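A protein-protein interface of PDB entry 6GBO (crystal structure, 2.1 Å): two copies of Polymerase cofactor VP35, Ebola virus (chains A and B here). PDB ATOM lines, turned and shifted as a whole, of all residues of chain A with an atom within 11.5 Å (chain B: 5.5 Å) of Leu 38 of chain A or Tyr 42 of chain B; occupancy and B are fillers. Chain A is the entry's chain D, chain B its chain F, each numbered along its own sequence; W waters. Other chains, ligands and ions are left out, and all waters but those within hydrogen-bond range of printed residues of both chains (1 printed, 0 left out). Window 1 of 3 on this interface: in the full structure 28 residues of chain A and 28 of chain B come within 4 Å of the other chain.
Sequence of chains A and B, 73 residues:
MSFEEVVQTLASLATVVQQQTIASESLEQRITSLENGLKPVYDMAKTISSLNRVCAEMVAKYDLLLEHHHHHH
Of the 18 printed residues of chain A, 5 touch a printed residue of chain B.
Along chain A the printed residues that touch a printed residue of chain B span positions 34 to 44.
Hydrophobic or aromatic side chains of chain B that line the printed part of chain A: Tyr 42 and Ala 45.
Along chain B the printed residues that touch a printed residue of chain A span positions 42 to 46.
Among the printed residues, no Asp or Glu carboxylate lies within 4 Å of a Lys or Arg side-chain nitrogen of the other chain.
Gln 29 of chain A touches none of the printed residues of chain B.
Printed residues of chain B within 4 Å of Leu 34 of chain A: Tyr 42 (2.7 Å).
Printed residues of chain B within 4 Å of Gly 37 of chain A: Tyr 42.
Leu 38 of chain A touches just one residue of chain B: Tyr 42 (3.4 Å).
Of the printed residues of chain B, Pro 40 of chain A touches Ala 45 (3.8 Å) and Lys 46 (3.8 Å).
Ala 45 of chain A touches none of the printed residues of chain B.
No residue of chain A comes within 4 Å of Leu 38 of chain B.
No residue of chain A comes within 4 Å of Pro 40 of chain B.
No residue of chain A comes within 4 Å of Val 41 of chain B.
Of chain A, only Leu 34, Gly 37 and Leu 38 come within 4 Å of Tyr 42 of chain B.
No residue of chain A comes within 4 Å of Asp 43 of chain B.
Ala 45 of chain B touches just these residues of chain A: Pro 40 and Met 44.
The nearest printed residue of chain B that does not touch Leu 38 of chain A is Leu 38 of chain B (6.0 Å).
The nearest printed residue of chain B that does not touch Gly 37 of chain A is Lys 46 of chain B (6.6 Å).
Leu 38 of chain A touches Tyr 42 of chain B, but with the chains exchanged Tyr 42 of chain A does not touch Leu 38 of chain B (11.6 Å).
Pro 40 of chain A touches Ala 45 of chain B, but with the chains exchanged Ala 45 of chain A does not touch Pro 40 of chain B (13.6 Å).
Pro 40 of chain A touches Lys 46 of chain B, but with the chains exchanged Lys 46 of chain A does not touch Pro 40 of chain B (16.3 Å).
Met 44 of chain A touches Ala 45 of chain B, but with the chains exchanged Ala 45 of chain A does not touch Met 44 of chain B (9.4 Å).
Positions printed for both chains: 38, 39, 40, 41, 42, 43, 44, 45 and 46.
Of the 6 pairs that touch across the chains among the printed residues, none has its exchanged pair printed and touching as well.
Water W1 lies within hydrogen-bond range of the backbone carbonyl oxygen of Pro 40 of chain A (2.7 Å) and the backbone carbonyl oxygen of Ala 45 of chain B (3.4 Å).
O of Leu 34 of chain A lies within hydrogen-bond range of OH of Tyr 42 of chain B (2.7 Å).
Among the printed residues, pairs that only touch across the chains: Gly 37 of chain A with Tyr 42 of chain B (3.2 Å), Leu 38 of chain A with Tyr 42 of chain B (3.4 Å), Met 44 of chain A with Ala 45 of chain B (3.5 Å), Pro 40 of chain A with Ala 45 of chain B (3.8 Å) and Pro 40 of chain A with Lys 46 of chain B (3.8 Å).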
ATOM      1  N   GLN A  29      15.151  20.844  -7.776  1.00  0.00           N
ATOM      2  CA  GLN A  29      14.254  21.700  -7.011  1.00  0.00           C
ATOM      3  C   GLN A  29      13.112  20.905  -6.364  1.00  0.00           C
ATOM      4  O   GLN A  29      12.681  21.221  -5.275  1.00  0.00           O
ATOM      5  CB  GLN A  29      13.717  22.850  -7.856  1.00  0.00           C
ATOM      6  CG  GLN A  29      14.807  23.828  -8.303  1.00  0.00           C
ATOM      7  CD  GLN A  29      15.358  24.692  -7.172  1.00  0.00           C
ATOM      8  OE1 GLN A  29      15.054  24.492  -5.979  1.00  0.00           O
ATOM      9  NE2 GLN A  29      16.188  25.666  -7.541  1.00  0.00           N
ATOM     10  N   ARG A  30      12.642  19.867  -7.025  1.00  0.00           N
ATOM     11  CA  ARG A  30      11.623  18.996  -6.450  1.00  0.00           C
ATOM     12  C   ARG A  30      12.156  18.237  -5.208  1.00  0.00           C
ATOM     13  O   ARG A  30      11.445  18.066  -4.211  1.00  0.00           O
ATOM     14  CB  ARG A  30      11.111  18.027  -7.519  1.00  0.00           C
ATOM     15  CG  ARG A  30      10.123  18.670  -8.481  1.00  0.00           C
ATOM     16  CD  ARG A  30       9.835  17.792  -9.684  1.00  0.00           C
ATOM     17  NE  ARG A  30       8.973  16.669  -9.343  1.00  0.00           N
ATOM     18  CZ  ARG A  30       8.648  15.685 -10.178  1.00  0.00           C
ATOM     19  NH1 ARG A  30       9.120  15.675 -11.412  1.00  0.00           N
ATOM     20  NH2 ARG A  30       7.834  14.714  -9.780  1.00  0.00           N
ATOM     21  N   ILE A  31      13.412  17.804  -5.254  1.00  0.00           N
ATOM     22  CA  ILE A  31      14.002  17.125  -4.107  1.00  0.00           C
ATOM     23  C   ILE A  31      14.242  18.103  -2.961  1.00  0.00           C
ATOM     24  O   ILE A  31      13.911  17.811  -1.825  1.00  0.00           O
ATOM     25  CB  ILE A  31      15.247  16.326  -4.492  1.00  0.00           C
ATOM     26  CG1 ILE A  31      14.799  15.081  -5.225  1.00  0.00           C
ATOM     27  CG2 ILE A  31      16.041  15.881  -3.270  1.00  0.00           C
ATOM     28  CD1 ILE A  31      14.137  14.045  -4.326  1.00  0.00           C
ATOM     29  N   THR A  32      14.739  19.288  -3.279  1.00  0.00           N
ATOM     30  CA  THR A  32      14.872  20.335  -2.286  1.00  0.00           C
ATOM     31  C   THR A  32      13.540  20.618  -1.559  1.00  0.00           C
ATOM     32  O   THR A  32      13.550  20.785  -0.329  1.00  0.00           O
ATOM     33  CB  THR A  32      15.469  21.607  -2.914  1.00  0.00           C
ATOM     34  OG1 THR A  32      16.761  21.297  -3.465  1.00  0.00           O
ATOM     35  CG2 THR A  32      15.630  22.720  -1.907  1.00  0.00           C
ATOM     36  N   SER A  33      12.412  20.681  -2.284  1.00  0.00           N
ATOM     37  CA  SER A  33      11.113  20.952  -1.646  1.00  0.00           C
ATOM     38  C   SER A  33      10.703  19.823  -0.708  1.00  0.00           C
ATOM     39  O   SER A  33      10.154  20.078   0.351  1.00  0.00           O
ATOM     40  CB  SER A  33      10.002  21.187  -2.661  1.00  0.00           C
ATOM     41  OG  SER A  33      10.238  22.373  -3.362  1.00  0.00           O
ATOM     42  N   LEU A  34      10.968  18.589  -1.118  1.00  0.00           N
ATOM     43  CA  LEU A  34      10.803  17.428  -0.258  1.00  0.00           C
ATOM     44  C   LEU A  34      11.664  17.492   0.981  1.00  0.00           C
ATOM     45  O   LEU A  34      11.203  17.160   2.078  1.00  0.00           O
ATOM     46  CB  LEU A  34      11.082  16.129  -0.995  1.00  0.00           C
ATOM     47  CG  LEU A  34      10.030  15.746  -2.023  1.00  0.00           C
ATOM     48  CD1 LEU A  34      10.492  14.503  -2.762  1.00  0.00           C
ATOM     49  CD2 LEU A  34       8.657  15.522  -1.387  1.00  0.00           C
ATOM     50  N   GLU A  35      12.907  17.915   0.832  1.00  0.00           N
ATOM     51  CA  GLU A  35      13.749  18.125   1.995  1.00  0.00           C
ATOM     52  C   GLU A  35      13.269  19.271   2.872  1.00  0.00           C
ATOM     53  O   GLU A  35      13.356  19.182   4.081  1.00  0.00           O
ATOM     54  CB  GLU A  35      15.188  18.347   1.592  1.00  0.00           C
ATOM     55  CG  GLU A  35      15.770  17.086   0.999  1.00  0.00           C
ATOM     56  CD  GLU A  35      17.078  17.314   0.291  1.00  0.00           C
ATOM     57  OE1 GLU A  35      17.365  18.463  -0.075  1.00  0.00           O
ATOM     58  OE2 GLU A  35      17.803  16.325   0.093  1.00  0.00           O
ATOM     59  N   ASN A  36      12.786  20.353   2.273  1.00  0.00           N
ATOM     60  CA  ASN A  36      12.194  21.421   3.049  1.00  0.00           C
ATOM     61  C   ASN A  36      10.980  20.948   3.877  1.00  0.00           C
ATOM     62  O   ASN A  36      10.696  21.524   4.942  1.00  0.00           O
ATOM     63  CB  ASN A  36      11.741  22.563   2.142  1.00  0.00           C
ATOM     64  CG  ASN A  36      12.892  23.434   1.671  1.00  0.00           C
ATOM     65  OD1 ASN A  36      13.946  23.496   2.300  1.00  0.00           O
ATOM     66  ND2 ASN A  36      12.685  24.121   0.564  1.00  0.00           N
ATOM     67  N   GLY A  37      10.264  19.942   3.362  1.00  0.00           N
ATOM     68  CA  GLY A  37       9.110  19.370   4.059  1.00  0.00           C
ATOM     69  C   GLY A  37       9.454  18.457   5.253  1.00  0.00           C
ATOM     70  O   GLY A  37       8.553  17.991   5.922  1.00  0.00           O
ATOM     71  N   LEU A  38      10.738  18.206   5.519  1.00  0.00           N
ATOM     72  CA  LEU A  38      11.155  17.472   6.714  1.00  0.00           C
ATOM     73  C   LEU A  38      11.035  18.255   8.024  1.00  0.00           C
ATOM     74  O   LEU A  38      11.209  17.698   9.110  1.00  0.00           O
ATOM     75  CB  LEU A  38      12.593  16.995   6.586  1.00  0.00           C
ATOM     76  CG  LEU A  38      12.815  15.910   5.551  1.00  0.00           C
ATOM     77  CD1 LEU A  38      14.287  15.896   5.158  1.00  0.00           C
ATOM     78  CD2 LEU A  38      12.379  14.559   6.090  1.00  0.00           C
ATOM     79  N   LYS A  39      10.784  19.542   7.920  1.00  0.00           N
ATOM     80  CA  LYS A  39      10.633  20.399   9.069  1.00  0.00           C
ATOM     81  C   LYS A  39       9.676  19.844  10.171  1.00  0.00           C
ATOM     82  O   LYS A  39      10.038  19.823  11.335  1.00  0.00           O
ATOM     83  CB  LYS A  39      10.185  21.765   8.555  1.00  0.00           C
ATOM     84  CG  LYS A  39       9.587  22.701   9.582  1.00  0.00           C
ATOM     85  CD  LYS A  39      10.646  23.313  10.437  1.00  0.00           C
ATOM     86  CE  LYS A  39      10.063  24.525  11.154  1.00  0.00           C
ATOM     87  NZ  LYS A  39      10.677  24.638  12.483  1.00  0.00           N
ATOM     88  N   PRO A  40       8.451  19.421   9.811  1.00  0.00           N
ATOM     89  CA  PRO A  40       7.597  18.872  10.878  1.00  0.00           C
ATOM     90  C   PRO A  40       8.162  17.621  11.552  1.00  0.00           C
ATOM     91  O   PRO A  40       7.766  17.305  12.672  1.00  0.00           O
ATOM     92  CB  PRO A  40       6.279  18.547  10.162  1.00  0.00           C
ATOM     93  CG  PRO A  40       6.491  18.864   8.712  1.00  0.00           C
ATOM     94  CD  PRO A  40       7.665  19.787   8.623  1.00  0.00           C
ATOM     95  N   VAL A  41       9.042  16.904  10.859  1.00  0.00           N
ATOM     96  CA  VAL A  41       9.709  15.770  11.432  1.00  0.00           C
ATOM     97  C   VAL A  41      10.651  16.253  12.539  1.00  0.00           C
ATOM     98  O   VAL A  41      10.633  15.700  13.644  1.00  0.00           O
ATOM     99  CB  VAL A  41      10.448  14.936  10.391  1.00  0.00           C
ATOM    100  CG1 VAL A  41      11.156  13.776  11.056  1.00  0.00           C
ATOM    101  CG2 VAL A  41       9.476  14.412   9.327  1.00  0.00           C
ATOM    102  N   TYR A  42      11.443  17.285  12.247  1.00  0.00           N
ATOM    103  CA  TYR A  42      12.308  17.895  13.223  1.00  0.00           C
ATOM    104  C   TYR A  42      11.496  18.442  14.407  1.00  0.00           C
ATOM    105  O   TYR A  42      11.825  18.169  15.560  1.00  0.00           O
ATOM    106  CB  TYR A  42      13.156  18.999  12.570  1.00  0.00           C
ATOM    107  CG  TYR A  42      13.900  19.845  13.553  1.00  0.00           C
ATOM    108  CD1 TYR A  42      15.129  19.430  14.070  1.00  0.00           C
ATOM    109  CD2 TYR A  42      13.394  21.083  13.963  1.00  0.00           C
ATOM    110  CE1 TYR A  42      15.823  20.207  14.983  1.00  0.00           C
ATOM    111  CE2 TYR A  42      14.071  21.865  14.884  1.00  0.00           C
ATOM    112  CZ  TYR A  42      15.288  21.419  15.388  1.00  0.00           C
ATOM    113  OH  TYR A  42      15.978  22.207  16.288  1.00  0.00           O
ATOM    114  N   ASP A  43      10.426  19.190  14.134  1.00  0.00           N
ATOM    115  CA  ASP A  43       9.616  19.781  15.205  1.00  0.00           C
ATOM    116  C   ASP A  43       8.944  18.740  16.095  1.00  0.00           C
ATOM    117  O   ASP A  43       8.794  18.955  17.316  1.00  0.00           O
ATOM    118  CB  ASP A  43       8.562  20.717  14.641  1.00  0.00           C
ATOM    119  CG  ASP A  43       9.168  21.932  13.969  1.00  0.00           C
ATOM    120  OD1 ASP A  43      10.242  22.387  14.419  1.00  0.00           O
ATOM    121  OD2 ASP A  43       8.582  22.428  12.992  1.00  0.00           O
ATOM    122  N   MET A  44       8.546  17.630  15.489  1.00  0.00           N
ATOM    123  CA  MET A  44       7.982  16.503  16.205  1.00  0.00           C
ATOM    124  C   MET A  44       9.023  15.886  17.154  1.00  0.00           C
ATOM    125  O   MET A  44       8.756  15.700  18.366  1.00  0.00           O
ATOM    126  CB  MET A  44       7.501  15.445  15.200  1.00  0.00           C
ATOM    127  CG  MET A  44       6.919  14.176  15.789  1.00  0.00           C
ATOM    128  SD  MET A  44       7.103  12.740  14.727  1.00  0.00           S
ATOM    129  CE  MET A  44       8.879  12.624  14.552  1.00  0.00           C
ATOM    130  N   ALA A  45      10.186  15.557  16.604  1.00  0.00           N
ATOM    131  CA  ALA A  45      11.253  14.914  17.354  1.00  0.00           C
ATOM    132  C   ALA A  45      11.694  15.742  18.550  1.00  0.00           C
ATOM    133  O   ALA A  45      11.995  15.186  19.590  1.00  0.00           O
ATOM    134  CB  ALA A  45      12.450  14.614  16.465  1.00  0.00           C
ATOM    135  N   LYS A  46      11.719  17.058  18.394  1.00  0.00           N
ATOM    136  CA  LYS A  46      12.087  17.956  19.461  1.00  0.00           C
ATOM    137  C   LYS A  46      11.215  17.878  20.722  1.00  0.00           C
ATOM    138  O   LYS A  46      11.643  18.338  21.774  1.00  0.00           O
ATOM    139  CB  LYS A  46      12.077  19.396  18.958  1.00  0.00           C
ATOM    140  CG  LYS A  46      13.313  19.761  18.166  1.00  0.00           C
ATOM    141  CD  LYS A  46      14.566  19.886  19.028  1.00  0.00           C
ATOM    142  CE  LYS A  46      14.360  20.808  20.234  1.00  0.00           C
ATOM    143  NZ  LYS A  46      15.622  21.117  20.961  1.00  0.00           N
ATOM    144  N   LEU B  38       5.748  10.676   0.735  1.00  0.00           N
ATOM    145  CA  LEU B  38       6.145  11.496   1.862  1.00  0.00           C
ATOM    146  C   LEU B  38       5.059  12.446   2.335  1.00  0.00           C
ATOM    147  O   LEU B  38       5.081  12.860   3.473  1.00  0.00           O
ATOM    148  CB  LEU B  38       7.424  12.277   1.571  1.00  0.00           C
ATOM    149  CG  LEU B  38       8.643  11.361   1.550  1.00  0.00           C
ATOM    150  CD1 LEU B  38       9.873  12.108   1.047  1.00  0.00           C
ATOM    151  CD2 LEU B  38       8.932  10.787   2.921  1.00  0.00           C
ATOM    152  N   LYS B  39       4.100  12.776   1.486  1.00  0.00           N
ATOM    153  CA  LYS B  39       2.983  13.618   1.918  1.00  0.00           C
ATOM    154  C   LYS B  39       2.255  13.074   3.180  1.00  0.00           C
ATOM    155  O   LYS B  39       2.135  13.793   4.150  1.00  0.00           O
ATOM    156  CB  LYS B  39       1.995  13.885   0.765  1.00  0.00           C
ATOM    157  CG  LYS B  39       0.857  14.818   1.157  1.00  0.00           C
ATOM    158  CD  LYS B  39       0.063  15.356  -0.024  1.00  0.00           C
ATOM    159  CE  LYS B  39      -0.419  16.781   0.295  1.00  0.00           C
ATOM    160  NZ  LYS B  39      -1.435  17.348  -0.624  1.00  0.00           N
ATOM    161  N   PRO B  40       1.785  11.803   3.184  1.00  0.00           N
ATOM    162  CA  PRO B  40       1.173  11.305   4.450  1.00  0.00           C
ATOM    163  C   PRO B  40       2.180  11.146   5.596  1.00  0.00           C
ATOM    164  O   PRO B  40       1.827  11.379   6.740  1.00  0.00           O
ATOM    165  CB  PRO B  40       0.578   9.958   4.061  1.00  0.00           C
ATOM    166  CG  PRO B  40       1.236   9.588   2.765  1.00  0.00           C
ATOM    167  CD  PRO B  40       1.550  10.874   2.071  1.00  0.00           C
ATOM    168  N   VAL B  41       3.435  10.834   5.267  1.00  0.00           N
ATOM    169  CA  VAL B  41       4.491  10.673   6.251  1.00  0.00           C
ATOM    170  C   VAL B  41       4.742  11.964   7.008  1.00  0.00           C
ATOM    171  O   VAL B  41       4.773  11.979   8.249  1.00  0.00           O
ATOM    172  CB  VAL B  41       5.797  10.148   5.592  1.00  0.00           C
ATOM    173  CG1 VAL B  41       6.964  10.145   6.571  1.00  0.00           C
ATOM    174  CG2 VAL B  41       5.589   8.740   5.091  1.00  0.00           C
ATOM    175  N   TYR B  42       4.882  13.052   6.277  1.00  0.00           N
ATOM    176  CA  TYR B  42       5.069  14.338   6.887  1.00  0.00           C
ATOM    177  C   TYR B  42       3.796  14.795   7.636  1.00  0.00           C
ATOM    178  O   TYR B  42       3.891  15.406   8.707  1.00  0.00           O
ATOM    179  CB  TYR B  42       5.439  15.398   5.829  1.00  0.00           C
ATOM    180  CG  TYR B  42       6.797  15.229   5.126  1.00  0.00           C
ATOM    181  CD1 TYR B  42       7.787  14.412   5.647  1.00  0.00           C
ATOM    182  CD2 TYR B  42       7.085  15.941   3.944  1.00  0.00           C
ATOM    183  CE1 TYR B  42       9.020  14.289   5.019  1.00  0.00           C
ATOM    184  CE2 TYR B  42       8.310  15.817   3.301  1.00  0.00           C
ATOM    185  CZ  TYR B  42       9.275  14.989   3.840  1.00  0.00           C
ATOM    186  OH  TYR B  42      10.508  14.856   3.243  1.00  0.00           O
ATOM    187  N   ASP B  43       2.623  14.532   7.053  1.00  0.00           N
ATOM    188  CA  ASP B  43       1.359  14.884   7.695  1.00  0.00           C
ATOM    189  C   ASP B  43       1.234  14.196   9.072  1.00  0.00           C
ATOM    190  O   ASP B  43       0.838  14.809  10.058  1.00  0.00           O
ATOM    191  CB  ASP B  43       0.186  14.495   6.773  1.00  0.00           C
ATOM    192  CG  ASP B  43      -0.972  15.433   6.874  1.00  0.00           C
ATOM    193  OD1 ASP B  43      -0.949  16.329   7.763  1.00  0.00           O
ATOM    194  OD2 ASP B  43      -1.918  15.279   6.063  1.00  0.00           O
ATOM    195  N   MET B  44       1.606  12.922   9.119  1.00  0.00           N
ATOM    196  CA  MET B  44       1.595  12.127  10.334  1.00  0.00           C
ATOM    197  C   MET B  44       2.530  12.666  11.400  1.00  0.00           C
ATOM    198  O   MET B  44       2.213  12.550  12.577  1.00  0.00           O
ATOM    199  CB  MET B  44       2.001  10.680  10.036  1.00  0.00           C
ATOM    200  CG  MET B  44       0.938   9.850   9.351  1.00  0.00           C
ATOM    201  SD  MET B  44       1.544   8.182   8.977  1.00  0.00           S
ATOM    202  CE  MET B  44       1.325   7.468  10.570  1.00  0.00           C
ATOM    203  N   ALA B  45       3.688  13.219  11.008  1.00  0.00           N
ATOM    204  CA  ALA B  45       4.593  13.816  11.983  1.00  0.00           C
ATOM    205  C   ALA B  45       3.908  14.970  12.697  1.00  0.00           C
ATOM    206  O   ALA B  45       4.098  15.148  13.903  1.00  0.00           O
ATOM    207  CB  ALA B  45       5.905  14.263  11.366  1.00  0.00           C
ATOM    208  N   LYS B  46       3.078  15.711  11.976  1.00  0.00           N
ATOM    209  CA  LYS B  46       2.263  16.759  12.592  1.00  0.00           C
ATOM    210  C   LYS B  46       1.253  16.216  13.595  1.00  0.00           C
ATOM    211  O   LYS B  46       1.015  16.829  14.628  1.00  0.00           O
ATOM    212  CB  LYS B  46       1.527  17.567  11.530  1.00  0.00           C
ATOM    213  CG  LYS B  46       2.470  18.388  10.657  1.00  0.00           C
ATOM    214  CD  LYS B  46       1.721  19.078   9.527  1.00  0.00           C
ATOM    215  CE  LYS B  46       2.707  19.634   8.518  1.00  0.00           C
ATOM    216  NZ  LYS B  46       1.992  20.218   7.372  1.00  0.00           N
HETATM  217  O   HOH W   1       5.395  18.306  13.612  1.00  0.00           O
